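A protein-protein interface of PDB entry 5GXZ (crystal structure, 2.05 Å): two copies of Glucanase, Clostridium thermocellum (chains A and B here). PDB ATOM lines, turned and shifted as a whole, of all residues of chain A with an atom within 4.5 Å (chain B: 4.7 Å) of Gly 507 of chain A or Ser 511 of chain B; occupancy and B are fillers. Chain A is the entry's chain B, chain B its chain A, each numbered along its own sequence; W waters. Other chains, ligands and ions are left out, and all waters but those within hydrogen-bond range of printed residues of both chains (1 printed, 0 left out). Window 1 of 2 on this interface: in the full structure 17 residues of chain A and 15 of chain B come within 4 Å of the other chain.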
ATOM      1  N   THR A 505      28.521 -15.333 -17.013  1.00  0.00           N
ATOM      2  CA  THR A 505      28.867 -14.408 -18.095  1.00  0.00           C
ATOM      3  C   THR A 505      28.304 -14.864 -19.458  1.00  0.00           C
ATOM      4  O   THR A 505      27.875 -16.014 -19.619  1.00  0.00           O
ATOM      5  CB  THR A 505      30.391 -14.203 -18.200  1.00  0.00           C
ATOM      6  OG1 THR A 505      31.027 -15.479 -18.324  1.00  0.00           O
ATOM      7  CG2 THR A 505      30.953 -13.485 -16.978  1.00  0.00           C
ATOM      8  N   ILE A 506      28.309 -13.942 -20.414  1.00  0.00           N
ATOM      9  CA  ILE A 506      27.866 -14.153 -21.795  1.00  0.00           C
ATOM     10  C   ILE A 506      29.049 -14.032 -22.750  1.00  0.00           C
ATOM     11  O   ILE A 506      29.818 -13.077 -22.639  1.00  0.00           O
ATOM     12  CB  ILE A 506      26.862 -13.060 -22.216  1.00  0.00           C
ATOM     13  CG1 ILE A 506      25.574 -13.185 -21.404  1.00  0.00           C
ATOM     14  CG2 ILE A 506      26.545 -13.205 -23.696  1.00  0.00           C
ATOM     15  CD1 ILE A 506      25.096 -14.610 -21.313  1.00  0.00           C
ATOM     16  N   GLY A 507      29.195 -14.987 -23.669  1.00  0.00           N
ATOM     17  CA  GLY A 507      30.287 -14.981 -24.644  1.00  0.00           C
ATOM     18  C   GLY A 507      29.867 -14.622 -26.059  1.00  0.00           C
ATOM     19  O   GLY A 507      30.725 -14.330 -26.902  1.00  0.00           O
ATOM     20  N   TYR A 508      28.554 -14.629 -26.301  1.00  0.00           N
ATOM     21  CA  TYR A 508      27.919 -14.248 -27.570  1.00  0.00           C
ATOM     22  C   TYR A 508      26.406 -14.247 -27.378  1.00  0.00           C
ATOM     23  O   TYR A 508      25.869 -15.198 -26.826  1.00  0.00           O
ATOM     24  CB  TYR A 508      28.283 -15.203 -28.712  1.00  0.00           C
ATOM     25  CG  TYR A 508      27.489 -14.961 -29.982  1.00  0.00           C
ATOM     26  CD1 TYR A 508      27.692 -13.822 -30.745  1.00  0.00           C
ATOM     27  CD2 TYR A 508      26.541 -15.885 -30.425  1.00  0.00           C
ATOM     28  CE1 TYR A 508      26.967 -13.596 -31.905  1.00  0.00           C
ATOM     29  CE2 TYR A 508      25.817 -15.673 -31.592  1.00  0.00           C
ATOM     30  CZ  TYR A 508      26.032 -14.526 -32.323  1.00  0.00           C
ATOM     31  OH  TYR A 508      25.321 -14.296 -33.478  1.00  0.00           O
ATOM     32  N   GLN A 553      25.724 -17.914 -26.123  1.00  0.00           N
ATOM     33  CA  GLN A 553      26.861 -18.590 -25.502  1.00  0.00           C
ATOM     34  C   GLN A 553      26.989 -18.027 -24.086  1.00  0.00           C
ATOM     35  O   GLN A 553      27.243 -16.833 -23.928  1.00  0.00           O
ATOM     36  CB  GLN A 553      28.150 -18.344 -26.304  1.00  0.00           C
ATOM     37  CG  GLN A 553      28.078 -18.892 -27.725  1.00  0.00           C
ATOM     38  CD  GLN A 553      29.335 -18.669 -28.540  1.00  0.00           C
ATOM     39  OE1 GLN A 553      30.378 -18.303 -28.012  1.00  0.00           O
ATOM     40  NE2 GLN A 553      29.247 -18.930 -29.837  1.00  0.00           N
ATOM     41  N   TYR B 508      22.515  -7.645 -28.031  1.00  0.00           N
ATOM     42  CA  TYR B 508      23.660  -8.129 -28.822  1.00  0.00           C
ATOM     43  C   TYR B 508      24.934  -8.082 -27.982  1.00  0.00           C
ATOM     44  O   TYR B 508      25.181  -7.076 -27.311  1.00  0.00           O
ATOM     45  CB  TYR B 508      23.878  -7.306 -30.106  1.00  0.00           C
ATOM     46  CG  TYR B 508      25.138  -7.694 -30.859  1.00  0.00           C
ATOM     47  CD1 TYR B 508      25.274  -8.959 -31.437  1.00  0.00           C
ATOM     48  CD2 TYR B 508      26.207  -6.809 -30.973  1.00  0.00           C
ATOM     49  CE1 TYR B 508      26.431  -9.327 -32.108  1.00  0.00           C
ATOM     50  CE2 TYR B 508      27.364  -7.171 -31.649  1.00  0.00           C
ATOM     51  CZ  TYR B 508      27.472  -8.431 -32.208  1.00  0.00           C
ATOM     52  OH  TYR B 508      28.613  -8.794 -32.879  1.00  0.00           O
ATOM     53  N   CYS B 509      25.727  -9.156 -28.034  1.00  0.00           N
ATOM     54  CA  CYS B 509      27.019  -9.232 -27.358  1.00  0.00           C
ATOM     55  C   CYS B 509      27.977  -9.891 -28.314  1.00  0.00           C
ATOM     56  O   CYS B 509      27.807 -11.062 -28.666  1.00  0.00           O
ATOM     57  CB  CYS B 509      27.012 -10.119 -26.112  1.00  0.00           C
ATOM     58  SG  CYS B 509      25.517 -10.008 -25.176  1.00  0.00           S
ATOM     59  N   GLU B 510      28.995  -9.132 -28.694  1.00  0.00           N
ATOM     60  CA  GLU B 510      29.949  -9.598 -29.690  1.00  0.00           C
ATOM     61  C   GLU B 510      30.575 -10.923 -29.303  1.00  0.00           C
ATOM     62  O   GLU B 510      31.005 -11.087 -28.160  1.00  0.00           O
ATOM     63  CB  GLU B 510      31.050  -8.558 -29.835  1.00  0.00           C
ATOM     64  CG  GLU B 510      32.217  -9.016 -30.670  1.00  0.00           C
ATOM     65  CD  GLU B 510      33.030  -7.835 -31.151  1.00  0.00           C
ATOM     66  OE1 GLU B 510      32.714  -6.696 -30.735  1.00  0.00           O
ATOM     67  OE2 GLU B 510      33.950  -8.055 -31.968  1.00  0.00           O
ATOM     68  N   SER B 511      30.625 -11.846 -30.260  1.00  0.00           N
ATOM     69  CA  SER B 511      31.226 -13.159 -30.057  1.00  0.00           C
ATOM     70  C   SER B 511      32.650 -13.160 -29.509  1.00  0.00           C
ATOM     71  O   SER B 511      33.530 -12.453 -30.015  1.00  0.00           O
ATOM     72  CB  SER B 511      31.248 -13.937 -31.366  1.00  0.00           C
ATOM     73  OG  SER B 511      31.639 -15.265 -31.087  1.00  0.00           O
ATOM     74  N   GLY B 512      32.872 -13.996 -28.499  1.00  0.00           N
ATOM     75  CA  GLY B 512      34.207 -14.179 -27.935  1.00  0.00           C
ATOM     76  C   GLY B 512      34.633 -13.148 -26.909  1.00  0.00           C
ATOM     77  O   GLY B 512      35.759 -13.184 -26.429  1.00  0.00           O
ATOM     78  N   MET B 513      33.738 -12.229 -26.562  1.00  0.00           N
ATOM     79  CA  MET B 513      34.026 -11.211 -25.556  1.00  0.00           C
ATOM     80  C   MET B 513      33.253 -11.527 -24.263  1.00  0.00           C
ATOM     81  O   MET B 513      32.137 -11.033 -24.061  1.00  0.00           O
ATOM     82  CB  MET B 513      33.673  -9.806 -26.074  1.00  0.00           C
ATOM     83  CG  MET B 513      34.401  -9.345 -27.341  1.00  0.00           C
ATOM     84  SD  MET B 513      36.205  -9.288 -27.241  1.00  0.00           S
ATOM     85  CE  MET B 513      36.426  -8.731 -25.556  1.00  0.00           C
ATOM     86  N   ASP B 514      33.855 -12.337 -23.396  1.00  0.00           N
ATOM     87  CA  ASP B 514      33.282 -12.746 -22.109  1.00  0.00           C
ATOM     88  C   ASP B 514      32.929 -11.515 -21.285  1.00  0.00           C
ATOM     89  O   ASP B 514      33.812 -10.744 -20.896  1.00  0.00           O
ATOM     90  CB  ASP B 514      34.285 -13.657 -21.383  1.00  0.00           C
ATOM     91  CG  ASP B 514      33.671 -14.451 -20.226  1.00  0.00           C
ATOM     92  OD1 ASP B 514      32.446 -14.704 -20.225  1.00  0.00           O
ATOM     93  OD2 ASP B 514      34.425 -14.850 -19.301  1.00  0.00           O
HETATM   94  O   HOH W   1      32.149 -16.195 -22.339  1.00  0.00           O
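1 position is printed for both chains.
Of the 10 pairs that touch across the chains among the printed residues, none has its exchanged pair printed and touching as well.
OG1 of Thr 505 of chain A is in hydrogen-bond range of OD1 of Asp 514 of chain B, at 2.5 Å.
The backbone NH (N) of Gly 512 of chain B lies within hydrogen-bond range of the backbone carbonyl oxygen (O) of Gly 507 of chain A (2.7 Å).
The backbone carbonyl oxygen of Gly 507 of chain A sits close to the backbone carbonyl oxygen of Glu 510 of chain B.
The backbone carbonyl oxygen of Ile 506 of chain A sits close to the backbone carbonyl oxygen of Met 513 of chain B, 3.4 Å away.
Among the printed residues, pairs that only touch across the chains: Ile 506 of chain A with Cys 509 of chain B (3.7 Å), Ile 506 of chain A with Asp 514 of chain B (3.5 Å), Gly 507 of chain A with Ser 511 of chain B (3.4 Å), Gly 507 of chain A with Met 513 of chain B (3.7 Å), Tyr 508 of chain A with Cys 509 of chain B (3.4 Å) and Tyr 508 of chain A with Ser 511 of chain B (3.6 Å).
Water W1 bridges the side-chain carboxylate of Asp 514 of chain B and the backbone NH of Gly 507 of chain A.
O of Gln 553 of chain A sits at hydrogen-bond distance from N of Gly 507 of chain A, at 2.7 Å.
The backbone carbonyl oxygen of Tyr 508 of chain A is in hydrogen-bond range of the backbone NH of Gln 553 of chain A (2.8 Å).
Printed residues of chain A that touch a printed residue of chain B: Thr 505, Ile 506, Gly 507 and Tyr 508.
Hydrophobic or aromatic side chains of chain A within 4 Å of the printed part of chain B: Ile 506 and Tyr 508.
Of the 7 printed residues of chain B, 6 touch a printed residue of chain A.
Printed residues of chain B that touch a printed residue of chain A: Cys 509, Glu 510, Ser 511, Gly 512, Met 513 and Asp 514.
Among the printed residues, 10 pairs touch across the chains.
Among the printed residues, no Asp or Glu carboxylate lies within 4 Å of a Lys or Arg side-chain nitrogen of the other chain.
Gly 507 of chain A touches just these residues of chain B: Glu 510 (3.5 Å), Ser 511 (3.4 Å), Gly 512 (2.7 Å) and Met 513 (3.7 Å).
Tyr 508 of chain B touches none of the printed residues of chain A.
Of the printed residues of chain A, Cys 509 of chain B touches Ile 506 (3.7 Å) and Tyr 508 (3.4 Å).
Of the printed residues of chain A, Glu 510 of chain B touches Gly 507.
Of the printed residues of chain A, Ser 511 of chain B touches Gly 507 (3.4 Å) and Tyr 508 (3.6 Å).
The nearest residue of chain B that does not touch Gly 507 of chain A is Asp 514 of chain B (4.5 Å).
The nearest printed residue of chain A that does not touch Ser 511 of chain B is Gln 553 of chain A (4.5 Å).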
